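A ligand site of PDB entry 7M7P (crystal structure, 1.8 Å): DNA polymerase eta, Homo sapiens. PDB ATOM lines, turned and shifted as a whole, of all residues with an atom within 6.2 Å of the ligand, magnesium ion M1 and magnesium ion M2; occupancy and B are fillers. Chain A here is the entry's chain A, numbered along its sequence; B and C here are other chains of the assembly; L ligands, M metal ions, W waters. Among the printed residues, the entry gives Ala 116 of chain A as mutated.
Within 4 Å of magnesium ion M2: Asp 16, Asp 118, Glu 119 and DA 9 of chain B.
Along chain A the residues within 4 Å of magnesium ion M2 span positions 16 to 119.
Magnesium ion M1 is bound by the side-chain carboxylate (OD1) of Asp 118 (2.0 Å), the side-chain carboxylate (OD1) of Asp 16 (2.1 Å), an oxygen (O3) of the ligand (2.1 Å), an oxygen (O2) of the ligand (2.2 Å), the backbone carbonyl oxygen (O) of Met 17 (2.2 Å) and an oxygen (O1) of the ligand (2.3 Å).
Merely in contact with magnesium ion M1: Lys 234 (3.8 Å).
Of the 24 residues printed, 4 come within 4 Å of magnesium ion M1.
Magnesium ion M2 is bound by the side-chain carboxylate of Asp 16 (2.1 Å), the side-chain carboxylate of Asp 118 (2.2 Å), water W8 (2.2 Å), an oxygen (O1) of the ligand (2.2 Å), the side-chain carboxylate of Glu 119 (2.2 Å) and O3' of DA 9 of chain B (2.3 Å).
Residues that only touch the ligand: Asp 18 (3.3 Å), Ile 51 (3.3 Å), Ala 52 (3.5 Å), Ile 117 (3.8 Å) and DT 5 of chain C (3.9 Å).
Hydrophobic or aromatic side chains within 4 Å of the ligand: Phe 20, Phe 21, Ala 52, Tyr 55 and Ile 117.
Of the 24 residues printed, 17 come within 4 Å of the ligand.
The side-chain amino group of Lys 234 lies within salt-bridge range of an oxygen (O6) of the ligand, 3.2 Å away.
The backbone NH (N) of Phe 20 lies within hydrogen-bond range of an oxygen (O5) of the ligand, at 3.3 Å.
The backbone NH (N) of Phe 21 sits at hydrogen-bond distance from an oxygen (O7) of the ligand.
The backbone NH (N) of Cys 19 is in hydrogen-bond range of an oxygen (O6) of the ligand (2.9 Å).
O4 of the ligand lies within salt-bridge range of NH1 of Arg 64, at 3.3 Å.
O4 of DT 4 of chain C lies within hydrogen-bond range of N3 of the ligand.
An oxygen (O9) of the ligand lies within salt-bridge range of the guanidinium group (NH1) of Arg 58 (3.2 Å).
An oxygen (O6) of the ligand sits at hydrogen-bond distance from the side-chain hydroxyl of Tyr 55 (2.6 Å).
Water W6 lies within hydrogen-bond range of an oxygen (O5) of the ligand (2.7 Å), the backbone NH (N) of Val 53 (2.8 Å) and the guanidinium group (NH2) of Arg 58 (2.9 Å).
Water W4 bridges an oxygen (O4) of the ligand (2.7 Å) and the guanidinium group (NH2) of Arg 64 (3.3 Å).
Water W1 lies within hydrogen-bond range of a nitrogen (N3) of the ligand (2.9 Å), the guanidinium group of Arg 64 (3.1 Å) and N7 of DA 9 of chain B (3.4 Å).
Water W7 bridges N3 of DA 9 of chain B (2.8 Å) and an oxygen (O10) of the ligand (3.3 Å).
The backbone carbonyl oxygen of Met 17 sits close to the side-chain amino group of Lys 234, 3.1 Å away.
The guanidinium group (NH1) of Arg 58 sits at hydrogen-bond distance from the side-chain hydroxyl (OH) of Tyr 55 (3.2 Å).
The guanidinium group of Arg 58 is in hydrogen-bond range of the backbone carbonyl oxygen of Val 53 (2.8 Å).
O2 of DT 4 of chain C is in hydrogen-bond range of NE2 of Gln 41, at 2.8 Å.
The side-chain amino group (NZ) of Lys 234 lies within salt-bridge range of the side-chain carboxylate (OD1) of Asp 18 (2.8 Å).
NZ of Lys 234 sits at hydrogen-bond distance from O of Asp 16 (3.1 Å).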
ATOM      1  N   ASP A  16     -27.018  -4.029 -38.800  1.00  0.00           N
ATOM      2  CA  ASP A  16     -26.462  -3.592 -37.525  1.00  0.00           C
ATOM      3  C   ASP A  16     -27.474  -2.693 -36.836  1.00  0.00           C
ATOM      4  O   ASP A  16     -27.852  -1.647 -37.373  1.00  0.00           O
ATOM      5  CB  ASP A  16     -25.145  -2.851 -37.695  1.00  0.00           C
ATOM      6  CG  ASP A  16     -24.499  -2.532 -36.372  1.00  0.00           C
ATOM      7  OD1 ASP A  16     -24.925  -1.573 -35.718  1.00  0.00           O
ATOM      8  OD2 ASP A  16     -23.589  -3.278 -35.977  1.00  0.00           O
ATOM      9  N   MET A  17     -27.842  -3.055 -35.614  1.00  0.00           N
ATOM     10  CA  MET A  17     -28.816  -2.280 -34.866  1.00  0.00           C
ATOM     11  C   MET A  17     -28.252  -0.907 -34.505  1.00  0.00           C
ATOM     12  O   MET A  17     -27.069  -0.748 -34.173  1.00  0.00           O
ATOM     13  CB  MET A  17     -29.174  -3.031 -33.588  1.00  0.00           C
ATOM     14  CG  MET A  17     -29.627  -4.477 -33.802  1.00  0.00           C
ATOM     15  SD  MET A  17     -30.977  -4.664 -35.001  1.00  0.00           S
ATOM     16  CE  MET A  17     -32.258  -3.777 -34.156  1.00  0.00           C
ATOM     17  N   ASP A  18     -29.108   0.104 -34.555  1.00  0.00           N
ATOM     18  CA  ASP A  18     -28.718   1.448 -34.138  1.00  0.00           C
ATOM     19  C   ASP A  18     -28.726   1.549 -32.616  1.00  0.00           C
ATOM     20  O   ASP A  18     -29.704   1.149 -31.967  1.00  0.00           O
ATOM     21  CB  ASP A  18     -29.678   2.465 -34.727  1.00  0.00           C
ATOM     22  CG  ASP A  18     -29.661   2.446 -36.255  1.00  0.00           C
ATOM     23  OD1 ASP A  18     -28.619   2.136 -36.854  1.00  0.00           O
ATOM     24  OD2 ASP A  18     -30.707   2.786 -36.856  1.00  0.00           O
ATOM     25  N   CYS A  19     -27.634   2.115 -32.043  1.00  0.00           N
ATOM     26  CA  CYS A  19     -27.413   2.314 -30.599  1.00  0.00           C
ATOM     27  C   CYS A  19     -28.152   1.224 -29.801  1.00  0.00           C
ATOM     28  O   CYS A  19     -29.044   1.504 -28.993  1.00  0.00           O
ATOM     29  CB  CYS A  19     -27.822   3.709 -30.093  1.00  0.00           C
ATOM     30  SG  CYS A  19     -29.482   4.320 -30.469  1.00  0.00           S
ATOM     31  N   PHE A  20     -27.753  -0.035 -30.025  1.00  0.00           N
ATOM     32  CA  PHE A  20     -28.565  -1.195 -29.664  1.00  0.00           C
ATOM     33  C   PHE A  20     -29.003  -1.242 -28.194  1.00  0.00           C
ATOM     34  O   PHE A  20     -30.201  -1.351 -27.894  1.00  0.00           O
ATOM     35  CB  PHE A  20     -27.835  -2.479 -30.058  1.00  0.00           C
ATOM     36  CG  PHE A  20     -28.641  -3.706 -29.838  1.00  0.00           C
ATOM     37  CD1 PHE A  20     -29.943  -3.772 -30.291  1.00  0.00           C
ATOM     38  CD2 PHE A  20     -28.102  -4.805 -29.183  1.00  0.00           C
ATOM     39  CE1 PHE A  20     -30.706  -4.905 -30.083  1.00  0.00           C
ATOM     40  CE2 PHE A  20     -28.868  -5.936 -28.985  1.00  0.00           C
ATOM     41  CZ  PHE A  20     -30.167  -5.993 -29.437  1.00  0.00           C
ATOM     42  N   PHE A  21     -28.060  -1.217 -27.243  1.00  0.00           N
ATOM     43  CA  PHE A  21     -28.462  -1.382 -25.837  1.00  0.00           C
ATOM     44  C   PHE A  21     -29.368  -0.227 -25.416  1.00  0.00           C
ATOM     45  O   PHE A  21     -30.305  -0.396 -24.615  1.00  0.00           O
ATOM     46  CB  PHE A  21     -27.250  -1.456 -24.908  1.00  0.00           C
ATOM     47  CG  PHE A  21     -26.458  -2.743 -25.014  1.00  0.00           C
ATOM     48  CD1 PHE A  21     -26.644  -3.626 -26.059  1.00  0.00           C
ATOM     49  CD2 PHE A  21     -25.489  -3.043 -24.051  1.00  0.00           C
ATOM     50  CE1 PHE A  21     -25.912  -4.804 -26.138  1.00  0.00           C
ATOM     51  CE2 PHE A  21     -24.745  -4.202 -24.140  1.00  0.00           C
ATOM     52  CZ  PHE A  21     -24.957  -5.086 -25.200  1.00  0.00           C
ATOM     53  N   VAL A  22     -29.111   0.966 -25.972  1.00  0.00           N
ATOM     54  CA  VAL A  22     -29.967   2.123 -25.678  1.00  0.00           C
ATOM     55  C   VAL A  22     -31.387   1.868 -26.182  1.00  0.00           C
ATOM     56  O   VAL A  22     -32.357   2.120 -25.466  1.00  0.00           O
ATOM     57  CB  VAL A  22     -29.363   3.406 -26.268  1.00  0.00           C
ATOM     58  CG1 VAL A  22     -30.410   4.524 -26.292  1.00  0.00           C
ATOM     59  CG2 VAL A  22     -28.124   3.824 -25.466  1.00  0.00           C
ATOM     60  N   GLN A  41     -22.441   0.693 -17.126  1.00  0.00           N
ATOM     61  CA  GLN A  41     -22.221  -0.475 -16.251  1.00  0.00           C
ATOM     62  C   GLN A  41     -21.479   0.016 -15.011  1.00  0.00           C
ATOM     63  O   GLN A  41     -20.549   0.800 -15.183  1.00  0.00           O
ATOM     64  CB  GLN A  41     -21.543  -1.675 -16.930  1.00  0.00           C
ATOM     65  CG  GLN A  41     -20.284  -1.394 -17.723  1.00  0.00           C
ATOM     66  CD  GLN A  41     -20.005  -2.610 -18.571  1.00  0.00           C
ATOM     67  OE1 GLN A  41     -20.845  -3.505 -18.726  1.00  0.00           O
ATOM     68  NE2 GLN A  41     -18.830  -2.648 -19.147  1.00  0.00           N
ATOM     69  N   ILE A  51     -21.424   2.215 -22.245  1.00  0.00           N
ATOM     70  CA  ILE A  51     -21.198   1.218 -23.287  1.00  0.00           C
ATOM     71  C   ILE A  51     -22.076   1.431 -24.521  1.00  0.00           C
ATOM     72  O   ILE A  51     -21.808   0.789 -25.554  1.00  0.00           O
ATOM     73  CB  ILE A  51     -21.355  -0.224 -22.754  1.00  0.00           C
ATOM     74  CG1 ILE A  51     -22.753  -0.474 -22.203  1.00  0.00           C
ATOM     75  CG2 ILE A  51     -20.286  -0.485 -21.671  1.00  0.00           C
ATOM     76  CD1 ILE A  51     -22.980  -1.939 -21.815  1.00  0.00           C
ATOM     77  N   ALA A  52     -23.095   2.296 -24.445  1.00  0.00           N
ATOM     78  CA  ALA A  52     -23.928   2.613 -25.616  1.00  0.00           C
ATOM     79  C   ALA A  52     -24.534   4.017 -25.459  1.00  0.00           C
ATOM     80  O   ALA A  52     -24.822   4.443 -24.338  1.00  0.00           O
ATOM     81  CB  ALA A  52     -25.027   1.559 -25.814  1.00  0.00           C
ATOM     82  N   VAL A  53     -24.731   4.706 -26.593  1.00  0.00           N
ATOM     83  CA  VAL A  53     -25.062   6.141 -26.590  1.00  0.00           C
ATOM     84  C   VAL A  53     -26.091   6.433 -27.677  1.00  0.00           C
ATOM     85  O   VAL A  53     -25.852   6.122 -28.846  1.00  0.00           O
ATOM     86  CB  VAL A  53     -23.794   7.003 -26.849  1.00  0.00           C
ATOM     87  CG1 VAL A  53     -24.070   8.500 -26.712  1.00  0.00           C
ATOM     88  CG2 VAL A  53     -22.637   6.604 -25.963  1.00  0.00           C
ATOM     89  N   TYR A  55     -28.236   8.642 -30.423  1.00  0.00           N
ATOM     90  CA  TYR A  55     -27.693   9.612 -31.376  1.00  0.00           C
ATOM     91  C   TYR A  55     -27.878  11.044 -30.875  1.00  0.00           C
ATOM     92  O   TYR A  55     -26.989  11.907 -31.073  1.00  0.00           O
ATOM     93  CB  TYR A  55     -28.315   9.408 -32.756  1.00  0.00           C
ATOM     94  CG  TYR A  55     -27.661   8.248 -33.442  1.00  0.00           C
ATOM     95  CD1 TYR A  55     -27.991   6.947 -33.110  1.00  0.00           C
ATOM     96  CD2 TYR A  55     -26.581   8.454 -34.301  1.00  0.00           C
ATOM     97  CE1 TYR A  55     -27.342   5.871 -33.705  1.00  0.00           C
ATOM     98  CE2 TYR A  55     -25.933   7.398 -34.881  1.00  0.00           C
ATOM     99  CZ  TYR A  55     -26.300   6.112 -34.579  1.00  0.00           C
ATOM    100  OH  TYR A  55     -25.645   5.055 -35.172  1.00  0.00           O
ATOM    101  N   ARG A  58     -24.896  11.536 -28.751  1.00  0.00           N
ATOM    102  CA  ARG A  58     -23.653  11.628 -29.505  1.00  0.00           C
ATOM    103  C   ARG A  58     -23.454  13.036 -30.045  1.00  0.00           C
ATOM    104  O   ARG A  58     -22.317  13.494 -30.208  1.00  0.00           O
ATOM    105  CB  ARG A  58     -23.668  10.648 -30.685  1.00  0.00           C
ATOM    106  CG  ARG A  58     -23.726   9.211 -30.258  1.00  0.00           C
ATOM    107  CD  ARG A  58     -23.802   8.280 -31.434  1.00  0.00           C
ATOM    108  NE  ARG A  58     -24.258   6.945 -31.027  1.00  0.00           N
ATOM    109  CZ  ARG A  58     -24.094   5.853 -31.758  1.00  0.00           C
ATOM    110  NH1 ARG A  58     -23.497   5.930 -32.936  1.00  0.00           N
ATOM    111  NH2 ARG A  58     -24.540   4.677 -31.311  1.00  0.00           N
ATOM    112  N   ARG A  64     -18.994   5.886 -26.277  1.00  0.00           N
ATOM    113  CA  ARG A  64     -18.597   4.650 -25.616  1.00  0.00           C
ATOM    114  C   ARG A  64     -17.261   4.798 -24.903  1.00  0.00           C
ATOM    115  O   ARG A  64     -16.353   5.475 -25.417  1.00  0.00           O
ATOM    116  CB  ARG A  64     -18.533   3.523 -26.656  1.00  0.00           C
ATOM    117  CG  ARG A  64     -17.785   2.254 -26.233  1.00  0.00           C
ATOM    118  CD  ARG A  64     -17.893   1.186 -27.324  1.00  0.00           C
ATOM    119  NE  ARG A  64     -17.486   1.705 -28.629  1.00  0.00           N
ATOM    120  CZ  ARG A  64     -18.021   1.342 -29.789  1.00  0.00           C
ATOM    121  NH1 ARG A  64     -19.021   0.449 -29.831  1.00  0.00           N
ATOM    122  NH2 ARG A  64     -17.581   1.871 -30.921  1.00  0.00           N
ATOM    123  N   ALA A 116     -22.038 -10.280 -34.252  1.00  0.00           N
ATOM    124  CA  ALA A 116     -21.897  -9.749 -32.900  1.00  0.00           C
ATOM    125  C   ALA A 116     -23.293  -9.650 -32.290  1.00  0.00           C
ATOM    126  O   ALA A 116     -24.293  -9.980 -32.943  1.00  0.00           O
ATOM    127  CB  ALA A 116     -21.166  -8.390 -32.908  1.00  0.00           C
ATOM    128  N   ILE A 117     -23.350  -9.195 -31.031  1.00  0.00           N
ATOM    129  CA  ILE A 117     -24.632  -9.185 -30.320  1.00  0.00           C
ATOM    130  C   ILE A 117     -25.704  -8.426 -31.093  1.00  0.00           C
ATOM    131  O   ILE A 117     -26.881  -8.783 -31.047  1.00  0.00           O
ATOM    132  CB  ILE A 117     -24.501  -8.620 -28.886  1.00  0.00           C
ATOM    133  CG1 ILE A 117     -25.748  -8.990 -28.082  1.00  0.00           C
ATOM    134  CG2 ILE A 117     -24.394  -7.105 -28.889  1.00  0.00           C
ATOM    135  CD1 ILE A 117     -25.563  -8.949 -26.545  1.00  0.00           C
ATOM    136  N   ASP A 118     -25.295  -7.472 -31.943  1.00  0.00           N
ATOM    137  CA  ASP A 118     -26.297  -6.642 -32.613  1.00  0.00           C
ATOM    138  C   ASP A 118     -26.097  -6.603 -34.121  1.00  0.00           C
ATOM    139  O   ASP A 118     -26.645  -5.720 -34.796  1.00  0.00           O
ATOM    140  CB  ASP A 118     -26.266  -5.194 -32.087  1.00  0.00           C
ATOM    141  CG  ASP A 118     -25.262  -4.282 -32.849  1.00  0.00           C
ATOM    142  OD1 ASP A 118     -25.578  -3.107 -33.070  1.00  0.00           O
ATOM    143  OD2 ASP A 118     -24.136  -4.747 -33.173  1.00  0.00           O
ATOM    144  N   GLU A 119     -25.374  -7.570 -34.670  1.00  0.00           N
ATOM    145  CA  GLU A 119     -25.248  -7.547 -36.122  1.00  0.00           C
ATOM    146  C   GLU A 119     -25.116  -8.945 -36.687  1.00  0.00           C
ATOM    147  O   GLU A 119     -24.543  -9.851 -36.054  1.00  0.00           O
ATOM    148  CB  GLU A 119     -24.076  -6.693 -36.590  1.00  0.00           C
ATOM    149  CG  GLU A 119     -22.725  -7.260 -36.318  1.00  0.00           C
ATOM    150  CD  GLU A 119     -21.705  -6.151 -36.289  1.00  0.00           C
ATOM    151  OE1 GLU A 119     -21.090  -5.936 -37.349  1.00  0.00           O
ATOM    152  OE2 GLU A 119     -21.615  -5.435 -35.275  1.00  0.00           O
ATOM    153  N   LYS A 234     -25.719   5.435 -41.221  1.00  0.00           N
ATOM    154  CA  LYS A 234     -26.355   5.269 -39.916  1.00  0.00           C
ATOM    155  C   LYS A 234     -26.780   6.619 -39.352  1.00  0.00           C
ATOM    156  O   LYS A 234     -26.034   7.600 -39.482  1.00  0.00           O
ATOM    157  CB  LYS A 234     -25.388   4.609 -38.931  1.00  0.00           C
ATOM    158  CG  LYS A 234     -25.366   3.122 -38.953  1.00  0.00           C
ATOM    159  CD  LYS A 234     -24.593   2.527 -37.771  1.00  0.00           C
ATOM    160  CE  LYS A 234     -24.942   1.054 -37.606  1.00  0.00           C
ATOM    161  NZ  LYS A 234     -26.108   0.823 -36.689  1.00  0.00           N
ATOM    162  N   PRO A 235     -27.918   6.691 -38.642  1.00  0.00           N
ATOM    163  CA  PRO A 235     -28.758   5.526 -38.338  1.00  0.00           C
ATOM    164  C   PRO A 235     -29.992   5.433 -39.232  1.00  0.00           C
ATOM    165  O   PRO A 235     -30.307   6.352 -39.988  1.00  0.00           O
ATOM    166  CB  PRO A 235     -29.208   5.803 -36.905  1.00  0.00           C
ATOM    167  CG  PRO A 235     -29.382   7.319 -36.913  1.00  0.00           C
ATOM    168  CD  PRO A 235     -28.304   7.858 -37.821  1.00  0.00           C
ATOM    169  P    DA B   9     -16.038  -3.437 -34.808  1.00  0.00           P
ATOM    170  OP1  DA B   9     -16.832  -2.888 -35.910  1.00  0.00           O
ATOM    171  OP2  DA B   9     -15.370  -2.481 -33.907  1.00  0.00           O
ATOM    172  O5'  DA B   9     -16.924  -4.460 -33.950  1.00  0.00           O
ATOM    173  C5'  DA B   9     -18.020  -5.392 -34.282  1.00  0.00           C
ATOM    174  C4'  DA B   9     -19.029  -5.435 -33.144  1.00  0.00           C
ATOM    175  O4'  DA B   9     -18.366  -5.887 -31.918  1.00  0.00           O
ATOM    176  C3'  DA B   9     -19.702  -4.107 -32.818  1.00  0.00           C
ATOM    177  O3'  DA B   9     -21.087  -4.362 -32.587  1.00  0.00           O
ATOM    178  C2'  DA B   9     -18.974  -3.627 -31.545  1.00  0.00           C
ATOM    179  C1'  DA B   9     -18.549  -4.924 -30.882  1.00  0.00           C
ATOM    180  N9   DA B   9     -17.289  -4.821 -30.129  1.00  0.00           N
ATOM    181  C8   DA B   9     -16.106  -4.271 -30.546  1.00  0.00           C
ATOM    182  N7   DA B   9     -15.148  -4.327 -29.656  1.00  0.00           N
ATOM    183  C5   DA B   9     -15.725  -4.955 -28.574  1.00  0.00           C
ATOM    184  C6   DA B   9     -15.246  -5.307 -27.293  1.00  0.00           C
ATOM    185  N6   DA B   9     -13.988  -5.075 -26.880  1.00  0.00           N
ATOM    186  N1   DA B   9     -16.091  -5.907 -26.455  1.00  0.00           N
ATOM    187  C2   DA B   9     -17.341  -6.153 -26.862  1.00  0.00           C
ATOM    188  N3   DA B   9     -17.922  -5.870 -28.027  1.00  0.00           N
ATOM    189  C4   DA B   9     -17.060  -5.266 -28.848  1.00  0.00           C
ATOM    190  P    DT C   3      -9.125   3.689 -17.483  1.00  0.00           P
ATOM    191  OP1  DT C   3      -7.686   3.383 -17.653  1.00  0.00           O
ATOM    192  OP2  DT C   3      -9.627   5.083 -17.657  1.00  0.00           O
ATOM    193  O5'  DT C   3      -9.950   2.728 -18.473  1.00  0.00           O
ATOM    194  C5'  DT C   3     -11.299   3.051 -18.815  1.00  0.00           C
ATOM    195  C4'  DT C   3     -12.153   1.790 -18.873  1.00  0.00           C
ATOM    196  O4'  DT C   3     -12.779   1.682 -20.169  1.00  0.00           O
ATOM    197  C3'  DT C   3     -11.390   0.498 -18.710  1.00  0.00           C
ATOM    198  O3'  DT C   3     -12.272  -0.524 -18.273  1.00  0.00           O
ATOM    199  C2'  DT C   3     -10.902   0.229 -20.131  1.00  0.00           C
ATOM    200  C1'  DT C   3     -12.051   0.779 -20.979  1.00  0.00           C
ATOM    201  N1   DT C   3     -11.589   1.491 -22.195  1.00  0.00           N
ATOM    202  C2   DT C   3     -12.302   1.362 -23.369  1.00  0.00           C
ATOM    203  O2   DT C   3     -13.309   0.667 -23.464  1.00  0.00           O
ATOM    204  N3   DT C   3     -11.797   2.062 -24.430  1.00  0.00           N
ATOM    205  C4   DT C   3     -10.663   2.869 -24.437  1.00  0.00           C
ATOM    206  O4   DT C   3     -10.288   3.465 -25.446  1.00  0.00           O
ATOM    207  C5   DT C   3      -9.964   2.970 -23.181  1.00  0.00           C
ATOM    208  C7   DT C   3      -8.730   3.816 -23.068  1.00  0.00           C
ATOM    209  C6   DT C   3     -10.459   2.279 -22.131  1.00  0.00           C
ATOM    210  P    DT C   4     -11.913  -1.418 -16.989  1.00  0.00           P
ATOM    211  OP1  DT C   4     -11.792  -0.534 -15.802  1.00  0.00           O
ATOM    212  OP2  DT C   4     -10.801  -2.300 -17.394  1.00  0.00           O
ATOM    213  O5'  DT C   4     -13.193  -2.331 -16.799  1.00  0.00           O
ATOM    214  C5'  DT C   4     -14.460  -1.746 -16.584  1.00  0.00           C
ATOM    215  C4'  DT C   4     -15.554  -2.677 -17.094  1.00  0.00           C
ATOM    216  O4'  DT C   4     -15.769  -2.452 -18.496  1.00  0.00           O
ATOM    217  C3'  DT C   4     -15.257  -4.163 -16.952  1.00  0.00           C
ATOM    218  O3'  DT C   4     -16.433  -4.798 -16.544  1.00  0.00           O
ATOM    219  C2'  DT C   4     -14.850  -4.587 -18.363  1.00  0.00           C
ATOM    220  C1'  DT C   4     -15.768  -3.691 -19.176  1.00  0.00           C
ATOM    221  N1   DT C   4     -15.333  -3.429 -20.592  1.00  0.00           N
ATOM    222  C2   DT C   4     -16.289  -3.425 -21.576  1.00  0.00           C
ATOM    223  O2   DT C   4     -17.456  -3.661 -21.351  1.00  0.00           O
ATOM    224  N3   DT C   4     -15.826  -3.161 -22.830  1.00  0.00           N
ATOM    225  C4   DT C   4     -14.521  -2.884 -23.206  1.00  0.00           C
ATOM    226  O4   DT C   4     -14.210  -2.649 -24.366  1.00  0.00           O
ATOM    227  C5   DT C   4     -13.557  -2.893 -22.120  1.00  0.00           C
ATOM    228  C7   DT C   4     -12.102  -2.612 -22.395  1.00  0.00           C
ATOM    229  C6   DT C   4     -14.001  -3.151 -20.879  1.00  0.00           C
ATOM    230  P    DT C   5     -16.460  -6.356 -16.233  1.00  0.00           P
ATOM    231  OP1  DT C   5     -17.375  -6.544 -15.084  1.00  0.00           O
ATOM    232  OP2  DT C   5     -15.082  -6.873 -16.168  1.00  0.00           O
ATOM    233  O5'  DT C   5     -17.163  -6.955 -17.536  1.00  0.00           O
ATOM    234  C5'  DT C   5     -18.510  -6.627 -17.835  1.00  0.00           C
ATOM    235  C4'  DT C   5     -18.951  -7.366 -19.073  1.00  0.00           C
ATOM    236  O4'  DT C   5     -18.272  -6.801 -20.224  1.00  0.00           O
ATOM    237  C3'  DT C   5     -18.635  -8.872 -19.065  1.00  0.00           C
ATOM    238  O3'  DT C   5     -19.761  -9.598 -19.537  1.00  0.00           O
ATOM    239  C2'  DT C   5     -17.422  -8.968 -20.007  1.00  0.00           C
ATOM    240  C1'  DT C   5     -17.745  -7.848 -21.004  1.00  0.00           C
ATOM    241  N1   DT C   5     -16.592  -7.338 -21.778  1.00  0.00           N
ATOM    242  C2   DT C   5     -16.790  -7.013 -23.101  1.00  0.00           C
ATOM    243  O2   DT C   5     -17.859  -7.135 -23.663  1.00  0.00           O
ATOM    244  N3   DT C   5     -15.673  -6.540 -23.748  1.00  0.00           N
ATOM    245  C4   DT C   5     -14.415  -6.355 -23.218  1.00  0.00           C
ATOM    246  O4   DT C   5     -13.478  -5.930 -23.884  1.00  0.00           O
ATOM    247  C5   DT C   5     -14.277  -6.714 -21.814  1.00  0.00           C
ATOM    248  C7   DT C   5     -12.955  -6.548 -21.126  1.00  0.00           C
ATOM    249  C6   DT C   5     -15.360  -7.176 -21.173  1.00  0.00           C
HETATM  250  N1  LIG L   1     -17.650  -3.040 -24.817  1.00  0.00           N
HETATM  251  C1  LIG L   1     -18.853  -3.427 -24.394  1.00  0.00           C
HETATM  252  N2  LIG L   1     -20.006  -3.438 -25.050  1.00  0.00           N
HETATM  253  C2  LIG L   1     -19.849  -2.957 -26.291  1.00  0.00           C
HETATM  254  C3  LIG L   1     -18.686  -2.506 -26.870  1.00  0.00           C
HETATM  255  C4  LIG L   1     -17.525  -2.548 -26.069  1.00  0.00           C
HETATM  256  N3  LIG L   1     -16.350  -2.148 -26.525  1.00  0.00           N
HETATM  257  N4  LIG L   1     -18.923  -2.079 -28.163  1.00  0.00           N
HETATM  258  C5  LIG L   1     -20.209  -2.280 -28.332  1.00  0.00           C
HETATM  259  N5  LIG L   1     -20.821  -2.817 -27.233  1.00  0.00           N
HETATM  260  P1  LIG L   1     -22.245  -1.324 -31.819  1.00  0.00           P
HETATM  261  P2  LIG L   1     -24.346   0.567 -31.222  1.00  0.00           P
HETATM  262  P3  LIG L   1     -24.397   2.067 -33.676  1.00  0.00           P
HETATM  263  C6  LIG L   1     -22.208  -3.191 -27.046  1.00  0.00           C
HETATM  264  O1  LIG L   1     -22.925  -1.888 -32.963  1.00  0.00           O
HETATM  265  O2  LIG L   1     -25.277  -0.439 -31.693  1.00  0.00           O
HETATM  266  O3  LIG L   1     -24.247   0.701 -34.208  1.00  0.00           O
HETATM  267  C7  LIG L   1     -23.150  -2.036 -26.711  1.00  0.00           C
HETATM  268  O4  LIG L   1     -20.742  -1.159 -32.119  1.00  0.00           O
HETATM  269  O5  LIG L   1     -24.646   0.931 -29.755  1.00  0.00           O
HETATM  270  O6  LIG L   1     -25.667   2.703 -34.099  1.00  0.00           O
HETATM  271  C8  LIG L   1     -23.760  -1.689 -28.066  1.00  0.00           C
HETATM  272  O7  LIG L   1     -25.060  -1.142 -27.965  1.00  0.00           O
HETATM  273  N6  LIG L   1     -22.810   0.126 -31.379  1.00  0.00           N
HETATM  274  O8  LIG L   1     -24.483   1.889 -32.097  1.00  0.00           O
HETATM  275  O9  LIG L   1     -23.200   2.920 -33.951  1.00  0.00           O
HETATM  276  C9  LIG L   1     -23.786  -3.042 -28.772  1.00  0.00           C
HETATM  277  O10 LIG L   1     -22.678  -3.801 -28.240  1.00  0.00           O
HETATM  278  C10 LIG L   1     -23.643  -2.945 -30.266  1.00  0.00           C
HETATM  279  O11 LIG L   1     -22.380  -2.326 -30.584  1.00  0.00           O
HETATM  280 MG    MG M   1     -24.961  -1.256 -33.685  1.00  0.00          MG
HETATM  281 MG    MG M   2     -22.531  -3.686 -34.218  1.00  0.00          MG
HETATM  282  O   HOH W   1     -16.338  -1.123 -29.288  1.00  0.00           O
HETATM  283  O   HOH W   2     -21.687  -5.553 -30.354  1.00  0.00           O
HETATM  284  O   HOH W   3     -21.068   3.057 -32.311  1.00  0.00           O
HETATM  285  O   HOH W   4     -18.756   0.101 -33.468  1.00  0.00           O
HETATM  286  O   HOH W   5     -21.898   0.180 -35.731  1.00  0.00           O
HETATM  287  O   HOH W   6     -23.808   3.297 -28.841  1.00  0.00           O
HETATM  288  O   HOH W   7     -20.666  -6.270 -27.495  1.00  0.00           O
HETATM  289  O   HOH W   8     -21.043  -2.259 -34.962  1.00  0.00           O
HETATM  290  O   HOH W   9     -21.673  -5.329 -23.549  1.00  0.00           O
